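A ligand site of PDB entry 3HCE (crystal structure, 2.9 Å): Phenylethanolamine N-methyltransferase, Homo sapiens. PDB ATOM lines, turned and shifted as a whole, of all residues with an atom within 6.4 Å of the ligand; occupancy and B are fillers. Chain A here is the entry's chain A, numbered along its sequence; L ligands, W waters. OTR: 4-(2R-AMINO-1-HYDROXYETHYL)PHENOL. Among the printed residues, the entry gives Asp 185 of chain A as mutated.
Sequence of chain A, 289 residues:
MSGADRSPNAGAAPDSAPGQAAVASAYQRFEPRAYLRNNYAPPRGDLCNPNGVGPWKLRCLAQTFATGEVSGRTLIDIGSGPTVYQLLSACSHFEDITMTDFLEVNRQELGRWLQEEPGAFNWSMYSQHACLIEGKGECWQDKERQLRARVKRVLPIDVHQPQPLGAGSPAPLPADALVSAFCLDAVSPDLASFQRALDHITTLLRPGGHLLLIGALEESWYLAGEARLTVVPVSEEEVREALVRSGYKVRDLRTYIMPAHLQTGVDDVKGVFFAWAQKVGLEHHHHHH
O4 of the ligand sits at hydrogen-bond distance from NZ of Lys 57 (2.8 Å). The side-chain carboxylate of Glu 219 is in salt-bridge range of a nitrogen (N8) of the ligand. OD2 of Asp 267 sits at hydrogen-bond distance from O7 of the ligand.
NH1 of Arg 44 sits at hydrogen-bond distance from OD1 of Asn 39 (3.0 Å). The side-chain hydroxyl (OH) of Tyr 40 lies within hydrogen-bond range of the side-chain hydroxyl (OH) of Tyr 85, at 3.0 Å. O of Tyr 35 sits close to ND2 of Asn 39 (3.3 Å). The side-chain carboxylate (OD2) of Asp 267 is in salt-bridge range of the guanidinium group (NH1) of Arg 44, at 2.8 Å. N of Val 269 sits close to OD1 of Asp 267, at 3.3 Å. NZ of Lys 57 sits close to OH of Tyr 40, 3.4 Å away.
Merely in contact with the ligand: Tyr 35, Asn 39, Tyr 40, Arg 44, Phe 182 and Tyr 222. Hydrophobic or aromatic side chains that line the ligand: Phe 182 and Tyr 222. Of the 22 residues printed, 9 come within 4 Å of the ligand. The nearest printed residue that does not touch the ligand is Val 53 (4.1 Å).
Water W1 lies within hydrogen-bond range of a nitrogen (N8) of the ligand (2.4 Å), the side-chain carboxylate (OD1) of Asp 185 (2.9 Å) and the side-chain carboxylate (OE2) of Glu 219 (3.0 Å).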
ATOM      1  N   TYR A  35     -28.480 -13.197 -32.385  1.00  0.00           N
ATOM      2  CA  TYR A  35     -27.473 -12.959 -31.370  1.00  0.00           C
ATOM      3  C   TYR A  35     -26.347 -12.098 -31.906  1.00  0.00           C
ATOM      4  O   TYR A  35     -26.005 -11.074 -31.323  1.00  0.00           O
ATOM      5  CB  TYR A  35     -26.882 -14.258 -30.887  1.00  0.00           C
ATOM      6  CG  TYR A  35     -25.752 -14.068 -29.912  1.00  0.00           C
ATOM      7  CD1 TYR A  35     -25.983 -13.588 -28.642  1.00  0.00           C
ATOM      8  CD2 TYR A  35     -24.462 -14.395 -30.261  1.00  0.00           C
ATOM      9  CE1 TYR A  35     -24.954 -13.445 -27.747  1.00  0.00           C
ATOM     10  CE2 TYR A  35     -23.423 -14.245 -29.326  1.00  0.00           C
ATOM     11  CZ  TYR A  35     -23.692 -13.762 -28.089  1.00  0.00           C
ATOM     12  OH  TYR A  35     -22.700 -13.610 -27.193  1.00  0.00           O
ATOM     13  N   ASN A  39     -25.175  -8.122 -30.760  1.00  0.00           N
ATOM     14  CA  ASN A  39     -23.977  -8.008 -29.948  1.00  0.00           C
ATOM     15  C   ASN A  39     -22.736  -7.752 -30.735  1.00  0.00           C
ATOM     16  O   ASN A  39     -21.720  -7.348 -30.180  1.00  0.00           O
ATOM     17  CB  ASN A  39     -23.792  -9.263 -29.108  1.00  0.00           C
ATOM     18  CG  ASN A  39     -24.817  -9.356 -28.060  1.00  0.00           C
ATOM     19  OD1 ASN A  39     -24.945  -8.452 -27.245  1.00  0.00           O
ATOM     20  ND2 ASN A  39     -25.601 -10.404 -28.085  1.00  0.00           N
ATOM     21  N   TYR A  40     -22.831  -7.982 -32.039  1.00  0.00           N
ATOM     22  CA  TYR A  40     -21.701  -7.777 -32.926  1.00  0.00           C
ATOM     23  C   TYR A  40     -22.021  -7.021 -34.236  1.00  0.00           C
ATOM     24  O   TYR A  40     -21.380  -7.242 -35.229  1.00  0.00           O
ATOM     25  CB  TYR A  40     -21.016  -9.124 -33.194  1.00  0.00           C
ATOM     26  CG  TYR A  40     -20.592  -9.809 -31.910  1.00  0.00           C
ATOM     27  CD1 TYR A  40     -21.442 -10.660 -31.231  1.00  0.00           C
ATOM     28  CD2 TYR A  40     -19.358  -9.548 -31.351  1.00  0.00           C
ATOM     29  CE1 TYR A  40     -21.067 -11.269 -30.052  1.00  0.00           C
ATOM     30  CE2 TYR A  40     -18.965 -10.156 -30.162  1.00  0.00           C
ATOM     31  CZ  TYR A  40     -19.810 -11.016 -29.528  1.00  0.00           C
ATOM     32  OH  TYR A  40     -19.415 -11.620 -28.363  1.00  0.00           O
ATOM     33  N   ARG A  44     -22.777  -1.997 -30.904  1.00  0.00           N
ATOM     34  CA  ARG A  44     -21.733  -2.660 -30.127  1.00  0.00           C
ATOM     35  C   ARG A  44     -20.657  -3.182 -31.067  1.00  0.00           C
ATOM     36  O   ARG A  44     -19.525  -3.481 -30.674  1.00  0.00           O
ATOM     37  CB  ARG A  44     -22.302  -3.796 -29.257  1.00  0.00           C
ATOM     38  CG  ARG A  44     -23.297  -3.312 -28.233  1.00  0.00           C
ATOM     39  CD  ARG A  44     -23.681  -4.429 -27.303  1.00  0.00           C
ATOM     40  NE  ARG A  44     -24.452  -3.939 -26.167  1.00  0.00           N
ATOM     41  CZ  ARG A  44     -24.975  -4.746 -25.260  1.00  0.00           C
ATOM     42  NH1 ARG A  44     -24.847  -6.065 -25.364  1.00  0.00           N
ATOM     43  NH2 ARG A  44     -25.666  -4.244 -24.238  1.00  0.00           N
ATOM     44  N   VAL A  53     -16.979  -1.508 -26.707  1.00  0.00           N
ATOM     45  CA  VAL A  53     -16.722  -2.766 -26.025  1.00  0.00           C
ATOM     46  C   VAL A  53     -15.950  -3.727 -26.910  1.00  0.00           C
ATOM     47  O   VAL A  53     -15.155  -4.539 -26.400  1.00  0.00           O
ATOM     48  CB  VAL A  53     -18.053  -3.410 -25.526  1.00  0.00           C
ATOM     49  CG1 VAL A  53     -19.034  -3.548 -26.655  1.00  0.00           C
ATOM     50  CG2 VAL A  53     -17.825  -4.767 -24.841  1.00  0.00           C
ATOM     51  N   GLY A  54     -16.155  -3.667 -28.224  1.00  0.00           N
ATOM     52  CA  GLY A  54     -15.378  -4.514 -29.113  1.00  0.00           C
ATOM     53  C   GLY A  54     -13.867  -4.223 -29.072  1.00  0.00           C
ATOM     54  O   GLY A  54     -13.006  -5.102 -28.914  1.00  0.00           O
ATOM     55  N   LYS A  57     -12.449  -5.570 -25.691  1.00  0.00           N
ATOM     56  CA  LYS A  57     -12.217  -7.008 -25.680  1.00  0.00           C
ATOM     57  C   LYS A  57     -10.963  -7.344 -26.472  1.00  0.00           C
ATOM     58  O   LYS A  57      -9.985  -7.876 -25.932  1.00  0.00           O
ATOM     59  CB  LYS A  57     -13.420  -7.786 -26.189  1.00  0.00           C
ATOM     60  CG  LYS A  57     -14.650  -7.775 -25.240  1.00  0.00           C
ATOM     61  CD  LYS A  57     -15.788  -8.673 -25.726  1.00  0.00           C
ATOM     62  CE  LYS A  57     -16.849  -7.930 -26.504  1.00  0.00           C
ATOM     63  NZ  LYS A  57     -17.870  -8.765 -27.210  1.00  0.00           N
ATOM     64  N   TYR A  85     -14.163 -13.813 -32.939  1.00  0.00           N
ATOM     65  CA  TYR A  85     -13.283 -12.719 -32.535  1.00  0.00           C
ATOM     66  C   TYR A  85     -12.377 -13.084 -31.374  1.00  0.00           C
ATOM     67  O   TYR A  85     -11.271 -12.566 -31.234  1.00  0.00           O
ATOM     68  CB  TYR A  85     -14.130 -11.511 -32.120  1.00  0.00           C
ATOM     69  CG  TYR A  85     -14.808 -11.700 -30.820  1.00  0.00           C
ATOM     70  CD1 TYR A  85     -14.198 -11.326 -29.648  1.00  0.00           C
ATOM     71  CD2 TYR A  85     -16.069 -12.304 -30.750  1.00  0.00           C
ATOM     72  CE1 TYR A  85     -14.819 -11.523 -28.422  1.00  0.00           C
ATOM     73  CE2 TYR A  85     -16.695 -12.496 -29.536  1.00  0.00           C
ATOM     74  CZ  TYR A  85     -16.065 -12.118 -28.379  1.00  0.00           C
ATOM     75  OH  TYR A  85     -16.683 -12.284 -27.181  1.00  0.00           O
ATOM     76  N   PHE A 182     -18.393 -15.379 -22.532  1.00  0.00           N
ATOM     77  CA  PHE A 182     -19.838 -15.253 -22.483  1.00  0.00           C
ATOM     78  C   PHE A 182     -20.495 -16.632 -22.520  1.00  0.00           C
ATOM     79  O   PHE A 182     -21.622 -16.813 -23.055  1.00  0.00           O
ATOM     80  CB  PHE A 182     -20.307 -14.381 -23.656  1.00  0.00           C
ATOM     81  CG  PHE A 182     -19.772 -12.996 -23.610  1.00  0.00           C
ATOM     82  CD1 PHE A 182     -18.926 -12.544 -24.582  1.00  0.00           C
ATOM     83  CD2 PHE A 182     -20.085 -12.157 -22.559  1.00  0.00           C
ATOM     84  CE1 PHE A 182     -18.423 -11.261 -24.510  1.00  0.00           C
ATOM     85  CE2 PHE A 182     -19.567 -10.879 -22.511  1.00  0.00           C
ATOM     86  CZ  PHE A 182     -18.742 -10.434 -23.485  1.00  0.00           C
ATOM     87  N   ASP A 185     -20.940 -17.750 -17.597  1.00  0.00           N
ATOM     88  CA  ASP A 185     -21.904 -16.801 -17.090  1.00  0.00           C
ATOM     89  C   ASP A 185     -23.283 -16.887 -17.742  1.00  0.00           C
ATOM     90  O   ASP A 185     -24.288 -16.501 -17.136  1.00  0.00           O
ATOM     91  CB  ASP A 185     -21.355 -15.382 -17.246  1.00  0.00           C
ATOM     92  CG  ASP A 185     -20.712 -15.147 -18.611  1.00  0.00           C
ATOM     93  OD1 ASP A 185     -21.231 -14.269 -19.334  1.00  0.00           O
ATOM     94  OD2 ASP A 185     -19.712 -15.840 -18.937  1.00  0.00           O
ATOM     95  N   ALA A 186     -23.322 -17.407 -18.968  1.00  0.00           N
ATOM     96  CA  ALA A 186     -24.535 -17.411 -19.770  1.00  0.00           C
ATOM     97  C   ALA A 186     -25.302 -18.708 -19.733  1.00  0.00           C
ATOM     98  O   ALA A 186     -26.457 -18.753 -20.161  1.00  0.00           O
ATOM     99  CB  ALA A 186     -24.208 -17.020 -21.212  1.00  0.00           C
ATOM    100  N   ALA A 216     -19.952 -11.608 -18.898  1.00  0.00           N
ATOM    101  CA  ALA A 216     -20.793 -10.475 -18.539  1.00  0.00           C
ATOM    102  C   ALA A 216     -20.767 -10.179 -17.012  1.00  0.00           C
ATOM    103  O   ALA A 216     -20.612 -11.072 -16.207  1.00  0.00           O
ATOM    104  CB  ALA A 216     -22.206 -10.722 -19.018  1.00  0.00           C
ATOM    105  N   GLU A 219     -25.152  -9.358 -15.442  1.00  0.00           N
ATOM    106  CA  GLU A 219     -26.159  -9.543 -16.484  1.00  0.00           C
ATOM    107  C   GLU A 219     -27.128 -10.579 -15.933  1.00  0.00           C
ATOM    108  O   GLU A 219     -26.690 -11.602 -15.424  1.00  0.00           O
ATOM    109  CB  GLU A 219     -25.530 -10.020 -17.812  1.00  0.00           C
ATOM    110  CG  GLU A 219     -26.572 -10.559 -18.752  1.00  0.00           C
ATOM    111  CD  GLU A 219     -26.143 -10.617 -20.190  1.00  0.00           C
ATOM    112  OE1 GLU A 219     -25.775  -9.583 -20.792  1.00  0.00           O
ATOM    113  OE2 GLU A 219     -26.195 -11.710 -20.781  1.00  0.00           O
ATOM    114  N   TRP A 221     -30.338 -11.354 -17.866  1.00  0.00           N
ATOM    115  CA  TRP A 221     -30.944 -11.961 -19.054  1.00  0.00           C
ATOM    116  C   TRP A 221     -30.299 -11.368 -20.272  1.00  0.00           C
ATOM    117  O   TRP A 221     -29.546 -10.376 -20.171  1.00  0.00           O
ATOM    118  CB  TRP A 221     -32.413 -11.641 -19.085  1.00  0.00           C
ATOM    119  CG  TRP A 221     -32.676 -10.175 -18.952  1.00  0.00           C
ATOM    120  CD1 TRP A 221     -32.731  -9.423 -17.773  1.00  0.00           C
ATOM    121  CD2 TRP A 221     -32.951  -9.266 -20.004  1.00  0.00           C
ATOM    122  NE1 TRP A 221     -33.026  -8.104 -18.052  1.00  0.00           N
ATOM    123  CE2 TRP A 221     -33.158  -7.984 -19.417  1.00  0.00           C
ATOM    124  CE3 TRP A 221     -33.006  -9.397 -21.388  1.00  0.00           C
ATOM    125  CZ2 TRP A 221     -33.431  -6.866 -20.190  1.00  0.00           C
ATOM    126  CZ3 TRP A 221     -33.259  -8.285 -22.155  1.00  0.00           C
ATOM    127  CH2 TRP A 221     -33.454  -7.039 -21.563  1.00  0.00           C
ATOM    128  N   TYR A 222     -30.587 -11.973 -21.424  1.00  0.00           N
ATOM    129  CA  TYR A 222     -30.239 -11.393 -22.731  1.00  0.00           C
ATOM    130  C   TYR A 222     -30.985 -12.137 -23.825  1.00  0.00           C
ATOM    131  O   TYR A 222     -31.139 -13.333 -23.749  1.00  0.00           O
ATOM    132  CB  TYR A 222     -28.731 -11.445 -22.992  1.00  0.00           C
ATOM    133  CG  TYR A 222     -28.200 -12.807 -23.370  1.00  0.00           C
ATOM    134  CD1 TYR A 222     -28.265 -13.255 -24.677  1.00  0.00           C
ATOM    135  CD2 TYR A 222     -27.645 -13.627 -22.441  1.00  0.00           C
ATOM    136  CE1 TYR A 222     -27.797 -14.502 -25.024  1.00  0.00           C
ATOM    137  CE2 TYR A 222     -27.196 -14.863 -22.777  1.00  0.00           C
ATOM    138  CZ  TYR A 222     -27.263 -15.300 -24.063  1.00  0.00           C
ATOM    139  OH  TYR A 222     -26.798 -16.549 -24.386  1.00  0.00           O
ATOM    140  N   LEU A 223     -31.456 -11.429 -24.839  1.00  0.00           N
ATOM    141  CA  LEU A 223     -32.216 -12.049 -25.925  1.00  0.00           C
ATOM    142  C   LEU A 223     -31.356 -12.519 -27.094  1.00  0.00           C
ATOM    143  O   LEU A 223     -30.256 -11.994 -27.314  1.00  0.00           O
ATOM    144  CB  LEU A 223     -33.271 -11.065 -26.454  1.00  0.00           C
ATOM    145  CG  LEU A 223     -34.154 -10.478 -25.358  1.00  0.00           C
ATOM    146  CD1 LEU A 223     -34.807  -9.155 -25.800  1.00  0.00           C
ATOM    147  CD2 LEU A 223     -35.179 -11.496 -24.988  1.00  0.00           C
ATOM    148  N   VAL A 231     -29.836 -15.731 -16.656  1.00  0.00           N
ATOM    149  CA  VAL A 231     -28.393 -15.804 -16.498  1.00  0.00           C
ATOM    150  C   VAL A 231     -28.036 -15.391 -15.086  1.00  0.00           C
ATOM    151  O   VAL A 231     -28.818 -14.686 -14.424  1.00  0.00           O
ATOM    152  CB  VAL A 231     -27.719 -14.915 -17.548  1.00  0.00           C
ATOM    153  CG1 VAL A 231     -26.295 -14.479 -17.093  1.00  0.00           C
ATOM    154  CG2 VAL A 231     -27.741 -15.627 -18.876  1.00  0.00           C
ATOM    155  N   MET A 258     -20.152  -1.078 -19.191  1.00  0.00           N
ATOM    156  CA  MET A 258     -20.901  -0.825 -20.384  1.00  0.00           C
ATOM    157  C   MET A 258     -21.438   0.610 -20.355  1.00  0.00           C
ATOM    158  O   MET A 258     -22.129   0.971 -19.431  1.00  0.00           O
ATOM    159  CB  MET A 258     -22.025  -1.823 -20.512  1.00  0.00           C
ATOM    160  CG  MET A 258     -22.672  -1.819 -21.902  1.00  0.00           C
ATOM    161  SD  MET A 258     -21.648  -2.555 -23.193  1.00  0.00           S
ATOM    162  CE  MET A 258     -21.335  -4.211 -22.631  1.00  0.00           C
ATOM    163  N   VAL A 266     -31.277  -5.441 -25.537  1.00  0.00           N
ATOM    164  CA  VAL A 266     -31.120  -6.851 -25.891  1.00  0.00           C
ATOM    165  C   VAL A 266     -30.625  -7.531 -24.649  1.00  0.00           C
ATOM    166  O   VAL A 266     -30.466  -8.734 -24.588  1.00  0.00           O
ATOM    167  CB  VAL A 266     -30.041  -7.099 -26.986  1.00  0.00           C
ATOM    168  CG1 VAL A 266     -30.343  -6.300 -28.252  1.00  0.00           C
ATOM    169  CG2 VAL A 266     -28.654  -6.823 -26.428  1.00  0.00           C
ATOM    170  N   ASP A 267     -30.344  -6.733 -23.626  1.00  0.00           N
ATOM    171  CA  ASP A 267     -29.924  -7.333 -22.387  1.00  0.00           C
ATOM    172  C   ASP A 267     -29.881  -6.286 -21.310  1.00  0.00           C
ATOM    173  O   ASP A 267     -30.384  -5.172 -21.490  1.00  0.00           O
ATOM    174  CB  ASP A 267     -28.567  -8.002 -22.514  1.00  0.00           C
ATOM    175  CG  ASP A 267     -27.519  -7.073 -22.968  1.00  0.00           C
ATOM    176  OD1 ASP A 267     -27.419  -5.982 -22.380  1.00  0.00           O
ATOM    177  OD2 ASP A 267     -26.797  -7.416 -23.945  1.00  0.00           O
ATOM    178  N   VAL A 269     -26.911  -6.345 -19.185  1.00  0.00           N
ATOM    179  CA  VAL A 269     -25.500  -6.320 -18.771  1.00  0.00           C
ATOM    180  C   VAL A 269     -25.023  -4.958 -18.317  1.00  0.00           C
ATOM    181  O   VAL A 269     -25.371  -3.961 -18.951  1.00  0.00           O
ATOM    182  CB  VAL A 269     -24.568  -6.740 -19.931  1.00  0.00           C
ATOM    183  CG1 VAL A 269     -24.786  -5.854 -21.095  1.00  0.00           C
ATOM    184  CG2 VAL A 269     -23.117  -6.661 -19.494  1.00  0.00           C
ATOM    185  N   VAL A 272     -18.281  -5.675 -18.396  1.00  0.00           N
ATOM    186  CA  VAL A 272     -17.712  -6.899 -18.990  1.00  0.00           C
ATOM    187  C   VAL A 272     -16.360  -7.202 -18.342  1.00  0.00           C
ATOM    188  O   VAL A 272     -15.575  -6.277 -18.012  1.00  0.00           O
ATOM    189  CB  VAL A 272     -17.519  -6.779 -20.525  1.00  0.00           C
ATOM    190  CG1 VAL A 272     -16.598  -7.822 -21.006  1.00  0.00           C
ATOM    191  CG2 VAL A 272     -18.835  -6.928 -21.235  1.00  0.00           C
HETATM  192  C2  OTR L   1     -22.536 -10.704 -25.099  1.00  0.00           C
HETATM  193  C3  OTR L   1     -21.499  -9.989 -25.702  1.00  0.00           C
HETATM  194  C4  OTR L   1     -21.240  -8.638 -25.390  1.00  0.00           C
HETATM  195  O4  OTR L   1     -20.214  -7.916 -26.035  1.00  0.00           O
HETATM  196  C5  OTR L   1     -22.008  -7.998 -24.452  1.00  0.00           C
HETATM  197  C6  OTR L   1     -23.028  -8.715 -23.856  1.00  0.00           C
HETATM  198  C1  OTR L   1     -23.311 -10.061 -24.149  1.00  0.00           C
HETATM  199  C7  OTR L   1     -24.483 -10.759 -23.440  1.00  0.00           C
HETATM  200  O7  OTR L   1     -25.727 -10.429 -24.077  1.00  0.00           O
HETATM  201  C8  OTR L   1     -24.164 -12.248 -23.491  1.00  0.00           C
HETATM  202  N8  OTR L   1     -24.278 -12.882 -22.196  1.00  0.00           N
HETATM  203  O   HOH W   1     -23.975 -13.499 -19.870  1.00  0.00           O
